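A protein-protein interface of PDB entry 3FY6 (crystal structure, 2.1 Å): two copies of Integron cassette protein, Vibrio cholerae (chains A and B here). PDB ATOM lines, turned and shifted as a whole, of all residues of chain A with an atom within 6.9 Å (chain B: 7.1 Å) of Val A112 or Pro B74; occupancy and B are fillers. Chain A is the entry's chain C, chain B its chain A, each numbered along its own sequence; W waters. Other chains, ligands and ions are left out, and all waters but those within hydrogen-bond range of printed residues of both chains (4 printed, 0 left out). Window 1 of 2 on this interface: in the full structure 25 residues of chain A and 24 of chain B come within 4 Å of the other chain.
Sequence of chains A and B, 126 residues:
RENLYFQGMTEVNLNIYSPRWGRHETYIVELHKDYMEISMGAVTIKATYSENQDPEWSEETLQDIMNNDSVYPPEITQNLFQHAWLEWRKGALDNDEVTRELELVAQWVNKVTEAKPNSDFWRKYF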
ATOM      1  N   GLN A  63     -10.448   1.694  -1.598  1.00  0.00           N
ATOM      2  CA  GLN A  63     -11.571   0.872  -2.054  1.00  0.00           C
ATOM      3  C   GLN A  63     -11.342   0.447  -3.499  1.00  0.00           C
ATOM      4  O   GLN A  63     -11.746  -0.648  -3.903  1.00  0.00           O
ATOM      5  CB  GLN A  63     -12.900   1.629  -1.952  1.00  0.00           C
ATOM      6  CG  GLN A  63     -13.343   1.943  -0.541  1.00  0.00           C
ATOM      7  CD  GLN A  63     -13.907   0.725   0.169  1.00  0.00           C
ATOM      8  OE1 GLN A  63     -14.445  -0.183  -0.467  1.00  0.00           O
ATOM      9  NE2 GLN A  63     -13.781   0.698   1.494  1.00  0.00           N
ATOM     10  N   TYR A  72     -14.359  -6.071  -0.034  1.00  0.00           N
ATOM     11  CA  TYR A  72     -15.295  -4.959   0.148  1.00  0.00           C
ATOM     12  C   TYR A  72     -15.371  -4.488   1.606  1.00  0.00           C
ATOM     13  O   TYR A  72     -16.317  -4.801   2.321  1.00  0.00           O
ATOM     14  CB  TYR A  72     -16.680  -5.347  -0.394  1.00  0.00           C
ATOM     15  CG  TYR A  72     -16.615  -5.877  -1.818  1.00  0.00           C
ATOM     16  CD1 TYR A  72     -16.498  -5.012  -2.899  1.00  0.00           C
ATOM     17  CD2 TYR A  72     -16.644  -7.241  -2.078  1.00  0.00           C
ATOM     18  CE1 TYR A  72     -16.423  -5.490  -4.198  1.00  0.00           C
ATOM     19  CE2 TYR A  72     -16.569  -7.726  -3.372  1.00  0.00           C
ATOM     20  CZ  TYR A  72     -16.454  -6.844  -4.425  1.00  0.00           C
ATOM     21  OH  TYR A  72     -16.384  -7.316  -5.712  1.00  0.00           O
ATOM     22  N   PRO A  73     -14.375  -3.708   2.044  1.00  0.00           N
ATOM     23  CA  PRO A  73     -14.315  -3.299   3.448  1.00  0.00           C
ATOM     24  C   PRO A  73     -15.197  -2.088   3.708  1.00  0.00           C
ATOM     25  O   PRO A  73     -15.659  -1.430   2.771  1.00  0.00           O
ATOM     26  CB  PRO A  73     -12.854  -2.880   3.633  1.00  0.00           C
ATOM     27  CG  PRO A  73     -12.284  -2.721   2.236  1.00  0.00           C
ATOM     28  CD  PRO A  73     -13.379  -2.994   1.234  1.00  0.00           C
ATOM     29  N   PRO A  74     -15.413  -1.768   4.985  1.00  0.00           N
ATOM     30  CA  PRO A  74     -16.201  -0.574   5.293  1.00  0.00           C
ATOM     31  C   PRO A  74     -15.557   0.657   4.665  1.00  0.00           C
ATOM     32  O   PRO A  74     -14.341   0.699   4.515  1.00  0.00           O
ATOM     33  CB  PRO A  74     -16.140  -0.505   6.814  1.00  0.00           C
ATOM     34  CG  PRO A  74     -15.904  -1.928   7.242  1.00  0.00           C
ATOM     35  CD  PRO A  74     -14.991  -2.489   6.197  1.00  0.00           C
ATOM     36  N   GLU A  75     -16.370   1.634   4.283  1.00  0.00           N
ATOM     37  CA  GLU A  75     -15.871   2.842   3.639  1.00  0.00           C
ATOM     38  C   GLU A  75     -14.851   3.591   4.510  1.00  0.00           C
ATOM     39  O   GLU A  75     -13.976   4.278   3.991  1.00  0.00           O
ATOM     40  CB  GLU A  75     -17.040   3.761   3.278  1.00  0.00           C
ATOM     41  CG  GLU A  75     -16.640   5.177   2.911  1.00  0.00           C
ATOM     42  CD  GLU A  75     -15.748   5.234   1.683  1.00  0.00           C
ATOM     43  OE1 GLU A  75     -15.917   4.381   0.781  1.00  0.00           O
ATOM     44  OE2 GLU A  75     -14.880   6.134   1.621  1.00  0.00           O
ATOM     45  N   ALA A 106      -6.529  -4.938   9.237  1.00  0.00           N
ATOM     46  CA  ALA A 106      -6.495  -6.003   8.237  1.00  0.00           C
ATOM     47  C   ALA A 106      -7.284  -7.211   8.719  1.00  0.00           C
ATOM     48  O   ALA A 106      -7.995  -7.855   7.944  1.00  0.00           O
ATOM     49  CB  ALA A 106      -5.058  -6.400   7.921  1.00  0.00           C
ATOM     50  N   GLN A 107      -7.147  -7.516  10.006  1.00  0.00           N
ATOM     51  CA  GLN A 107      -7.893  -8.613  10.615  1.00  0.00           C
ATOM     52  C   GLN A 107      -9.398  -8.366  10.491  1.00  0.00           C
ATOM     53  O   GLN A 107     -10.164  -9.270  10.175  1.00  0.00           O
ATOM     54  CB  GLN A 107      -7.515  -8.771  12.086  1.00  0.00           C
ATOM     55  CG  GLN A 107      -8.026 -10.061  12.706  1.00  0.00           C
ATOM     56  CD  GLN A 107      -7.644 -10.192  14.166  1.00  0.00           C
ATOM     57  OE1 GLN A 107      -7.971  -9.333  14.981  1.00  0.00           O
ATOM     58  NE2 GLN A 107      -6.951 -11.272  14.503  1.00  0.00           N
ATOM     59  N   TRP A 108      -9.811  -7.131  10.755  1.00  0.00           N
ATOM     60  CA  TRP A 108     -11.203  -6.746  10.592  1.00  0.00           C
ATOM     61  C   TRP A 108     -11.657  -6.959   9.148  1.00  0.00           C
ATOM     62  O   TRP A 108     -12.679  -7.580   8.905  1.00  0.00           O
ATOM     63  CB  TRP A 108     -11.397  -5.286  10.965  1.00  0.00           C
ATOM     64  CG  TRP A 108     -12.840  -4.881  11.064  1.00  0.00           C
ATOM     65  CD1 TRP A 108     -13.893  -5.656  11.473  1.00  0.00           C
ATOM     66  CD2 TRP A 108     -13.378  -3.593  10.776  1.00  0.00           C
ATOM     67  NE1 TRP A 108     -15.055  -4.925  11.447  1.00  0.00           N
ATOM     68  CE2 TRP A 108     -14.763  -3.652  11.028  1.00  0.00           C
ATOM     69  CE3 TRP A 108     -12.820  -2.388  10.331  1.00  0.00           C
ATOM     70  CZ2 TRP A 108     -15.595  -2.555  10.841  1.00  0.00           C
ATOM     71  CZ3 TRP A 108     -13.646  -1.304  10.151  1.00  0.00           C
ATOM     72  CH2 TRP A 108     -15.015  -1.391  10.405  1.00  0.00           C
ATOM     73  N   VAL A 109     -10.888  -6.443   8.196  1.00  0.00           N
ATOM     74  CA  VAL A 109     -11.236  -6.598   6.787  1.00  0.00           C
ATOM     75  C   VAL A 109     -11.393  -8.074   6.421  1.00  0.00           C
ATOM     76  O   VAL A 109     -12.359  -8.457   5.758  1.00  0.00           O
ATOM     77  CB  VAL A 109     -10.183  -5.952   5.889  1.00  0.00           C
ATOM     78  CG1 VAL A 109     -10.463  -6.264   4.420  1.00  0.00           C
ATOM     79  CG2 VAL A 109     -10.115  -4.445   6.153  1.00  0.00           C
ATOM     80  N   ASN A 110     -10.457  -8.905   6.869  1.00  0.00           N
ATOM     81  CA  ASN A 110     -10.540 -10.342   6.615  1.00  0.00           C
ATOM     82  C   ASN A 110     -11.768 -10.986   7.261  1.00  0.00           C
ATOM     83  O   ASN A 110     -12.364 -11.902   6.694  1.00  0.00           O
ATOM     84  CB  ASN A 110      -9.260 -11.051   7.070  1.00  0.00           C
ATOM     85  CG  ASN A 110      -8.058 -10.691   6.206  1.00  0.00           C
ATOM     86  OD1 ASN A 110      -6.909 -10.756   6.646  1.00  0.00           O
ATOM     87  ND2 ASN A 110      -8.325 -10.288   4.981  1.00  0.00           N
ATOM     88  N   LYS A 111     -12.137 -10.512   8.452  1.00  0.00           N
ATOM     89  CA  LYS A 111     -13.332 -11.016   9.139  1.00  0.00           C
ATOM     90  C   LYS A 111     -14.596 -10.643   8.378  1.00  0.00           C
ATOM     91  O   LYS A 111     -15.524 -11.439   8.270  1.00  0.00           O
ATOM     92  CB  LYS A 111     -13.431 -10.469  10.570  1.00  0.00           C
ATOM     93  CG  LYS A 111     -12.540 -11.178  11.590  1.00  0.00           C
ATOM     94  CD  LYS A 111     -12.864 -10.706  13.012  1.00  0.00           C
ATOM     95  CE  LYS A 111     -11.817 -11.147  14.023  1.00  0.00           C
ATOM     96  NZ  LYS A 111     -11.969 -10.410  15.319  1.00  0.00           N
ATOM     97  N   VAL A 112     -14.624  -9.417   7.868  1.00  0.00           N
ATOM     98  CA  VAL A 112     -15.723  -8.949   7.042  1.00  0.00           C
ATOM     99  C   VAL A 112     -15.866  -9.867   5.825  1.00  0.00           C
ATOM    100  O   VAL A 112     -16.958 -10.323   5.495  1.00  0.00           O
ATOM    101  CB  VAL A 112     -15.467  -7.507   6.584  1.00  0.00           C
ATOM    102  CG1 VAL A 112     -16.454  -7.092   5.508  1.00  0.00           C
ATOM    103  CG2 VAL A 112     -15.527  -6.557   7.792  1.00  0.00           C
ATOM    104  N   THR A 113     -14.749 -10.148   5.168  1.00  0.00           N
ATOM    105  CA  THR A 113     -14.761 -11.015   4.009  1.00  0.00           C
ATOM    106  C   THR A 113     -15.260 -12.408   4.403  1.00  0.00           C
ATOM    107  O   THR A 113     -16.158 -12.959   3.763  1.00  0.00           O
ATOM    108  CB  THR A 113     -13.371 -11.079   3.348  1.00  0.00           C
ATOM    109  OG1 THR A 113     -13.049  -9.786   2.822  1.00  0.00           O
ATOM    110  CG2 THR A 113     -13.368 -12.091   2.218  1.00  0.00           C
ATOM    111  N   GLU A 114     -14.694 -12.947   5.479  1.00  0.00           N
ATOM    112  CA  GLU A 114     -15.077 -14.258   6.000  1.00  0.00           C
ATOM    113  C   GLU A 114     -16.574 -14.367   6.306  1.00  0.00           C
ATOM    114  O   GLU A 114     -17.173 -15.427   6.124  1.00  0.00           O
ATOM    115  CB  GLU A 114     -14.281 -14.582   7.268  1.00  0.00           C
ATOM    116  CG  GLU A 114     -14.837 -15.757   8.069  1.00  0.00           C
ATOM    117  CD  GLU A 114     -14.310 -15.818   9.499  1.00  0.00           C
ATOM    118  OE1 GLU A 114     -13.476 -14.967   9.876  1.00  0.00           O
ATOM    119  OE2 GLU A 114     -14.736 -16.720  10.252  1.00  0.00           O
ATOM    120  N   ALA A 115     -17.174 -13.277   6.774  1.00  0.00           N
ATOM    121  CA  ALA A 115     -18.571 -13.324   7.205  1.00  0.00           C
ATOM    122  C   ALA A 115     -19.580 -12.969   6.111  1.00  0.00           C
ATOM    123  O   ALA A 115     -20.777 -12.841   6.398  1.00  0.00           O
ATOM    124  CB  ALA A 115     -18.779 -12.412   8.425  1.00  0.00           C
ATOM    125  N   LYS A 116     -19.120 -12.798   4.873  1.00  0.00           N
ATOM    126  CA  LYS A 116     -20.027 -12.444   3.779  1.00  0.00           C
ATOM    127  C   LYS A 116     -21.256 -13.356   3.758  1.00  0.00           C
ATOM    128  O   LYS A 116     -21.166 -14.536   4.111  1.00  0.00           O
ATOM    129  CB  LYS A 116     -19.329 -12.531   2.420  1.00  0.00           C
ATOM    130  CG  LYS A 116     -18.258 -11.488   2.191  1.00  0.00           C
ATOM    131  CD  LYS A 116     -17.986 -11.270   0.706  1.00  0.00           C
ATOM    132  CE  LYS A 116     -17.926 -12.562  -0.049  1.00  0.00           C
ATOM    133  NZ  LYS A 116     -17.117 -12.424  -1.296  1.00  0.00           N
ATOM    134  N   PRO A 117     -22.412 -12.814   3.347  1.00  0.00           N
ATOM    135  CA  PRO A 117     -23.600 -13.675   3.255  1.00  0.00           C
ATOM    136  C   PRO A 117     -23.315 -14.909   2.392  1.00  0.00           C
ATOM    137  O   PRO A 117     -22.636 -14.801   1.368  1.00  0.00           O
ATOM    138  CB  PRO A 117     -24.637 -12.765   2.595  1.00  0.00           C
ATOM    139  CG  PRO A 117     -24.224 -11.379   3.012  1.00  0.00           C
ATOM    140  CD  PRO A 117     -22.720 -11.397   3.080  1.00  0.00           C
ATOM    141  N   PHE A 126     -21.867 -12.039  -5.478  1.00  0.00           N
ATOM    142  CA  PHE A 126     -20.550 -11.509  -5.157  1.00  0.00           C
ATOM    143  C   PHE A 126     -19.800 -12.444  -4.220  1.00  0.00           C
ATOM    144  O   PHE A 126     -20.334 -13.473  -3.809  1.00  0.00           O
ATOM    145  CB  PHE A 126     -20.651 -10.089  -4.572  1.00  0.00           C
ATOM    146  CG  PHE A 126     -20.915 -10.042  -3.081  1.00  0.00           C
ATOM    147  CD1 PHE A 126     -20.080  -9.319  -2.242  1.00  0.00           C
ATOM    148  CD2 PHE A 126     -22.007 -10.702  -2.529  1.00  0.00           C
ATOM    149  CE1 PHE A 126     -20.320  -9.254  -0.868  1.00  0.00           C
ATOM    150  CE2 PHE A 126     -22.259 -10.646  -1.163  1.00  0.00           C
ATOM    151  CZ  PHE A 126     -21.421  -9.919  -0.328  1.00  0.00           C
ATOM    152  OXT PHE A 126     -18.645 -12.195  -3.866  1.00  0.00           O
ATOM    153  N   GLN B  63     -24.676   3.801   3.739  1.00  0.00           N
ATOM    154  CA  GLN B  63     -23.507   3.854   4.591  1.00  0.00           C
ATOM    155  C   GLN B  63     -23.524   5.125   5.448  1.00  0.00           C
ATOM    156  O   GLN B  63     -23.256   5.074   6.650  1.00  0.00           O
ATOM    157  CB  GLN B  63     -22.237   3.760   3.732  1.00  0.00           C
ATOM    158  CG  GLN B  63     -22.055   2.393   3.035  1.00  0.00           C
ATOM    159  CD  GLN B  63     -22.923   2.198   1.774  1.00  0.00           C
ATOM    160  OE1 GLN B  63     -23.213   3.149   1.040  1.00  0.00           O
ATOM    161  NE2 GLN B  63     -23.313   0.948   1.511  1.00  0.00           N
ATOM    162  N   TYR B  72     -20.426   0.909  10.677  1.00  0.00           N
ATOM    163  CA  TYR B  72     -19.538   1.043   9.522  1.00  0.00           C
ATOM    164  C   TYR B  72     -19.628  -0.213   8.676  1.00  0.00           C
ATOM    165  O   TYR B  72     -18.841  -1.143   8.840  1.00  0.00           O
ATOM    166  CB  TYR B  72     -18.099   1.312  10.007  1.00  0.00           C
ATOM    167  CG  TYR B  72     -18.091   2.485  10.955  1.00  0.00           C
ATOM    168  CD1 TYR B  72     -18.011   3.785  10.471  1.00  0.00           C
ATOM    169  CD2 TYR B  72     -18.269   2.301  12.323  1.00  0.00           C
ATOM    170  CE1 TYR B  72     -18.055   4.870  11.330  1.00  0.00           C
ATOM    171  CE2 TYR B  72     -18.313   3.378  13.190  1.00  0.00           C
ATOM    172  CZ  TYR B  72     -18.203   4.661  12.688  1.00  0.00           C
ATOM    173  OH  TYR B  72     -18.248   5.741  13.543  1.00  0.00           O
ATOM    174  N   PRO B  73     -20.610  -0.243   7.764  1.00  0.00           N
ATOM    175  CA  PRO B  73     -20.938  -1.422   6.965  1.00  0.00           C
ATOM    176  C   PRO B  73     -19.987  -1.514   5.789  1.00  0.00           C
ATOM    177  O   PRO B  73     -19.402  -0.505   5.407  1.00  0.00           O
ATOM    178  CB  PRO B  73     -22.343  -1.106   6.432  1.00  0.00           C
ATOM    179  CG  PRO B  73     -22.550   0.384   6.664  1.00  0.00           C
ATOM    180  CD  PRO B  73     -21.308   0.954   7.274  1.00  0.00           C
ATOM    181  N   PRO B  74     -19.828  -2.707   5.215  1.00  0.00           N
ATOM    182  CA  PRO B  74     -19.015  -2.797   3.998  1.00  0.00           C
ATOM    183  C   PRO B  74     -19.573  -1.833   2.948  1.00  0.00           C
ATOM    184  O   PRO B  74     -20.780  -1.584   2.913  1.00  0.00           O
ATOM    185  CB  PRO B  74     -19.207  -4.245   3.563  1.00  0.00           C
ATOM    186  CG  PRO B  74     -19.563  -4.978   4.847  1.00  0.00           C
ATOM    187  CD  PRO B  74     -20.379  -4.010   5.628  1.00  0.00           C
ATOM    188  N   GLU B  75     -18.706  -1.271   2.116  1.00  0.00           N
ATOM    189  CA  GLU B  75     -19.132  -0.253   1.160  1.00  0.00           C
ATOM    190  C   GLU B  75     -20.136  -0.795   0.127  1.00  0.00           C
ATOM    191  O   GLU B  75     -20.972  -0.053  -0.378  1.00  0.00           O
ATOM    192  CB  GLU B  75     -17.910   0.374   0.470  1.00  0.00           C
ATOM    193  CG  GLU B  75     -18.177   0.939  -0.928  1.00  0.00           C
ATOM    194  CD  GLU B  75     -19.001   2.221  -0.914  1.00  0.00           C
ATOM    195  OE1 GLU B  75     -18.879   2.998   0.058  1.00  0.00           O
ATOM    196  OE2 GLU B  75     -19.763   2.455  -1.881  1.00  0.00           O
ATOM    197  N   ILE B  76     -20.057  -2.090  -0.170  1.00  0.00           N
ATOM    198  CA  ILE B  76     -20.958  -2.717  -1.137  1.00  0.00           C
ATOM    199  C   ILE B  76     -22.387  -2.968  -0.613  1.00  0.00           C
ATOM    200  O   ILE B  76     -23.257  -3.420  -1.360  1.00  0.00           O
ATOM    201  CB  ILE B  76     -20.390  -4.063  -1.600  1.00  0.00           C
ATOM    202  CG1 ILE B  76     -21.050  -4.500  -2.913  1.00  0.00           C
ATOM    203  CG2 ILE B  76     -20.549  -5.117  -0.487  1.00  0.00           C
ATOM    204  CD1 ILE B  76     -20.482  -5.802  -3.483  1.00  0.00           C
ATOM    205  N   THR B  77     -22.627  -2.679   0.658  1.00  0.00           N
ATOM    206  CA  THR B  77     -23.930  -2.962   1.274  1.00  0.00           C
ATOM    207  C   THR B  77     -25.130  -2.396   0.488  1.00  0.00           C
ATOM    208  O   THR B  77     -26.122  -3.081   0.272  1.00  0.00           O
ATOM    209  CB  THR B  77     -23.967  -2.463   2.735  1.00  0.00           C
ATOM    210  OG1 THR B  77     -22.913  -3.099   3.471  1.00  0.00           O
ATOM    211  CG2 THR B  77     -25.314  -2.797   3.392  1.00  0.00           C
ATOM    212  N   GLN B  78     -25.037  -1.145   0.063  1.00  0.00           N
ATOM    213  CA  GLN B  78     -26.142  -0.502  -0.620  1.00  0.00           C
ATOM    214  C   GLN B  78     -26.427  -1.219  -1.929  1.00  0.00           C
ATOM    215  O   GLN B  78     -27.579  -1.398  -2.317  1.00  0.00           O
ATOM    216  CB  GLN B  78     -25.812   0.960  -0.895  1.00  0.00           C
ATOM    217  CG  GLN B  78     -26.858   1.695  -1.699  1.00  0.00           C
ATOM    218  CD  GLN B  78     -26.653   3.198  -1.635  1.00  0.00           C
ATOM    219  OE1 GLN B  78     -26.287   3.834  -2.623  1.00  0.00           O
ATOM    220  NE2 GLN B  78     -26.859   3.765  -0.461  1.00  0.00           N
ATOM    221  N   LEU B  80     -25.844  -4.347  -2.545  1.00  0.00           N
ATOM    222  CA  LEU B  80     -26.569  -5.582  -2.202  1.00  0.00           C
ATOM    223  C   LEU B  80     -28.070  -5.337  -2.061  1.00  0.00           C
ATOM    224  O   LEU B  80     -28.876  -6.101  -2.590  1.00  0.00           O
ATOM    225  CB  LEU B  80     -26.040  -6.209  -0.916  1.00  0.00           C
ATOM    226  CG  LEU B  80     -24.571  -6.631  -0.889  1.00  0.00           C
ATOM    227  CD1 LEU B  80     -24.355  -7.616   0.247  1.00  0.00           C
ATOM    228  CD2 LEU B  80     -24.138  -7.233  -2.219  1.00  0.00           C
ATOM    229  N   VAL B 105     -28.067  -9.810   4.793  1.00  0.00           N
ATOM    230  CA  VAL B 105     -27.205  -8.641   4.677  1.00  0.00           C
ATOM    231  C   VAL B 105     -27.121  -7.912   6.025  1.00  0.00           C
ATOM    232  O   VAL B 105     -26.043  -7.491   6.450  1.00  0.00           O
ATOM    233  CB  VAL B 105     -27.676  -7.673   3.596  1.00  0.00           C
ATOM    234  CG1 VAL B 105     -26.766  -6.455   3.571  1.00  0.00           C
ATOM    235  CG2 VAL B 105     -27.672  -8.362   2.237  1.00  0.00           C
ATOM    236  N   TRP B 108     -24.838  -9.768   8.259  1.00  0.00           N
ATOM    237  CA  TRP B 108     -23.451  -9.488   7.907  1.00  0.00           C
ATOM    238  C   TRP B 108     -22.989  -8.165   8.535  1.00  0.00           C
ATOM    239  O   TRP B 108     -21.930  -8.086   9.162  1.00  0.00           O
ATOM    240  CB  TRP B 108     -23.310  -9.405   6.387  1.00  0.00           C
ATOM    241  CG  TRP B 108     -21.891  -9.242   5.901  1.00  0.00           C
ATOM    242  CD1 TRP B 108     -20.762  -9.731   6.487  1.00  0.00           C
ATOM    243  CD2 TRP B 108     -21.470  -8.601   4.691  1.00  0.00           C
ATOM    244  NE1 TRP B 108     -19.657  -9.421   5.722  1.00  0.00           N
ATOM    245  CE2 TRP B 108     -20.065  -8.721   4.618  1.00  0.00           C
ATOM    246  CE3 TRP B 108     -22.140  -7.921   3.672  1.00  0.00           C
ATOM    247  CZ2 TRP B 108     -19.325  -8.185   3.573  1.00  0.00           C
ATOM    248  CZ3 TRP B 108     -21.401  -7.392   2.626  1.00  0.00           C
ATOM    249  CH2 TRP B 108     -20.014  -7.536   2.580  1.00  0.00           C
ATOM    250  N   VAL B 109     -23.782  -7.121   8.346  1.00  0.00           N
ATOM    251  CA  VAL B 109     -23.470  -5.836   8.947  1.00  0.00           C
ATOM    252  C   VAL B 109     -23.281  -6.001  10.458  1.00  0.00           C
ATOM    253  O   VAL B 109     -22.329  -5.464  11.024  1.00  0.00           O
ATOM    254  CB  VAL B 109     -24.548  -4.789   8.633  1.00  0.00           C
ATOM    255  CG1 VAL B 109     -24.311  -3.506   9.433  1.00  0.00           C
ATOM    256  CG2 VAL B 109     -24.569  -4.493   7.131  1.00  0.00           C
ATOM    257  N   LYS B 111     -22.294  -8.605  12.110  1.00  0.00           N
ATOM    258  CA  LYS B 111     -21.027  -9.285  12.366  1.00  0.00           C
ATOM    259  C   LYS B 111     -19.825  -8.338  12.215  1.00  0.00           C
ATOM    260  O   LYS B 111     -18.854  -8.424  12.961  1.00  0.00           O
ATOM    261  CB  LYS B 111     -20.866 -10.500  11.445  1.00  0.00           C
ATOM    262  CG  LYS B 111     -21.726 -11.695  11.851  1.00  0.00           C
ATOM    263  CD  LYS B 111     -21.503 -12.853  10.886  1.00  0.00           C
ATOM    264  CE  LYS B 111     -22.584 -13.925  10.993  1.00  0.00           C
ATOM    265  NZ  LYS B 111     -22.458 -14.930   9.889  1.00  0.00           N
ATOM    266  N   VAL B 112     -19.901  -7.453  11.231  1.00  0.00           N
ATOM    267  CA  VAL B 112     -18.864  -6.458  10.992  1.00  0.00           C
ATOM    268  C   VAL B 112     -18.706  -5.560  12.220  1.00  0.00           C
ATOM    269  O   VAL B 112     -17.601  -5.359  12.729  1.00  0.00           O
ATOM    270  CB  VAL B 112     -19.216  -5.617   9.755  1.00  0.00           C
ATOM    271  CG1 VAL B 112     -18.212  -4.459   9.566  1.00  0.00           C
ATOM    272  CG2 VAL B 112     -19.242  -6.521   8.513  1.00  0.00           C
ATOM    273  N   THR B 113     -19.832  -5.044  12.703  1.00  0.00           N
ATOM    274  CA  THR B 113     -19.860  -4.177  13.874  1.00  0.00           C
ATOM    275  C   THR B 113     -19.252  -4.882  15.082  1.00  0.00           C
ATOM    276  O   THR B 113     -18.397  -4.332  15.777  1.00  0.00           O
ATOM    277  CB  THR B 113     -21.309  -3.767  14.190  1.00  0.00           C
ATOM    278  OG1 THR B 113     -21.829  -3.010  13.089  1.00  0.00           O
ATOM    279  CG2 THR B 113     -21.377  -2.927  15.487  1.00  0.00           C
ATOM    280  N   ALA B 115     -17.180  -7.275  15.130  1.00  0.00           N
ATOM    281  CA  ALA B 115     -15.763  -7.564  14.939  1.00  0.00           C
ATOM    282  C   ALA B 115     -14.884  -6.316  14.814  1.00  0.00           C
ATOM    283  O   ALA B 115     -13.687  -6.423  14.609  1.00  0.00           O
ATOM    284  CB  ALA B 115     -15.574  -8.468  13.711  1.00  0.00           C
HETATM  285  O   HOH W   1     -11.606  -7.909  13.867  1.00  0.00           O
HETATM  286  O   HOH W   2     -19.253   1.824   4.455  1.00  0.00           O
HETATM  287  O   HOH W   3     -22.969 -12.933   8.053  1.00  0.00           O
HETATM  288  O   HOH W   4     -16.804  -1.929  -0.623  1.00  0.00           O
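Water W2 bridges O of Pro B73 (2.5 Å) and N of Glu A75 (2.9 Å). Water W1 lies within hydrogen-bond range of O of Ala B115 and NZ of Lys A111. Water W3 lies within hydrogen-bond range of O of Ala A115 and NZ of Lys B111. Water W4 lies within hydrogen-bond range of the side-chain amide oxygen (OE1) of Gln A63, the backbone NH (N) of Ile B76 and the backbone NH (N) of Glu B75.
Of the 18 printed residues of chain A, 12 touch a printed residue of chain B. Printed residues of chain A that touch a printed residue of chain B: Gln A63, Tyr A72, Pro A73, Pro A74, Glu A75, Trp A108, Lys A111, Val A112, Ala A115, Lys A116, Pro A117 and Phe A126. Printed residues of chain B that touch a printed residue of chain A: Tyr B72, Pro B73, Pro B74, Glu B75, Ile B76, Leu B80, Trp B108, Lys B111, Val B112 and Ala B115. Among the printed residues, no Asp or Glu carboxylate lies within 4 Å of a Lys or Arg side-chain nitrogen of the other chain.
Tyr A72 touches Ile B76. Tyr B72 touches Pro A74. Pro B73 touches Glu A75 (O to N, 3.9 Å). Trp A108 touches Ala B115. Lys A111 touches Ala B115. Pro B74 touches Val A112 (CG to CG1, 3.8 Å). CG2 of Val A112 touches CG2 of Val B112, 3.8 Å away. Ala A115 touches Trp B108 (O to CD1, 3.1 Å). Ala A115 touches Lys B111 (CB to CD, 3.7 Å). Lys A116 touches Trp B108 (N to NE1, 3.5 Å).
Pro B74 touches just these residues of chain A: Tyr A72 (3.2 Å), Pro A73 (3.8 Å), Pro A74 (3.8 Å) and Val A112 (3.8 Å). Of the printed residues of chain A, Glu B75 touches Gln A63 (3.6 Å), Pro A73 (3.1 Å) and Glu A75 (3.3 Å). Of the printed residues of chain B, Phe A126 touches Ile B76 (3.8 Å), Leu B80 (3.8 Å) and Trp B108 (3.9 Å). The nearest printed residue of chain B that does not touch Phe A126 is Pro B74 (6.8 Å).
NE2 of Gln B63 sits at hydrogen-bond distance from O of Glu B75 (3.2 Å). The side-chain amide nitrogen of Gln A63 sits at hydrogen-bond distance from the backbone carbonyl oxygen of Pro A73 (3.1 Å). The chain-end carboxylate of Phe A126 is in salt-bridge range of the side-chain amino group of Lys A116 (3.0 Å). The side-chain amide nitrogen (NE2) of Gln A63 is in hydrogen-bond range of the backbone carbonyl oxygen (O) of Pro A74 (3.1 Å). O of Pro B74 is in hydrogen-bond range of OG1 of Thr B77, 2.7 Å away.
Gln A63 touches Glu B75, but with the chains exchanged Glu A75 does not touch Gln B63 (5.2 Å). Glu A75 touches its own counterpart, Glu B75. Trp A108 touches Val B112, and with the chains exchanged Val A112 touches Trp B108. Trp A108 touches Ala B115, and with the chains exchanged Ala A115 touches Trp B108. Of the 23 pairs that touch across the chains among the printed residues, 15 have their exchanged pair printed and touching as well.
The indole nitrogen (NE1) of Trp A108 sits at hydrogen-bond distance from the backbone carbonyl oxygen (O) of Val B112 (2.9 Å). NE1 of Trp B108 sits at hydrogen-bond distance from O of Val A112, at 2.9 Å. The backbone NH (N) of Glu B75 sits at hydrogen-bond distance from the backbone carbonyl oxygen (O) of Pro A73. OE1 of Glu B75 lies close to OE1 of Glu A75 (3.3 Å).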
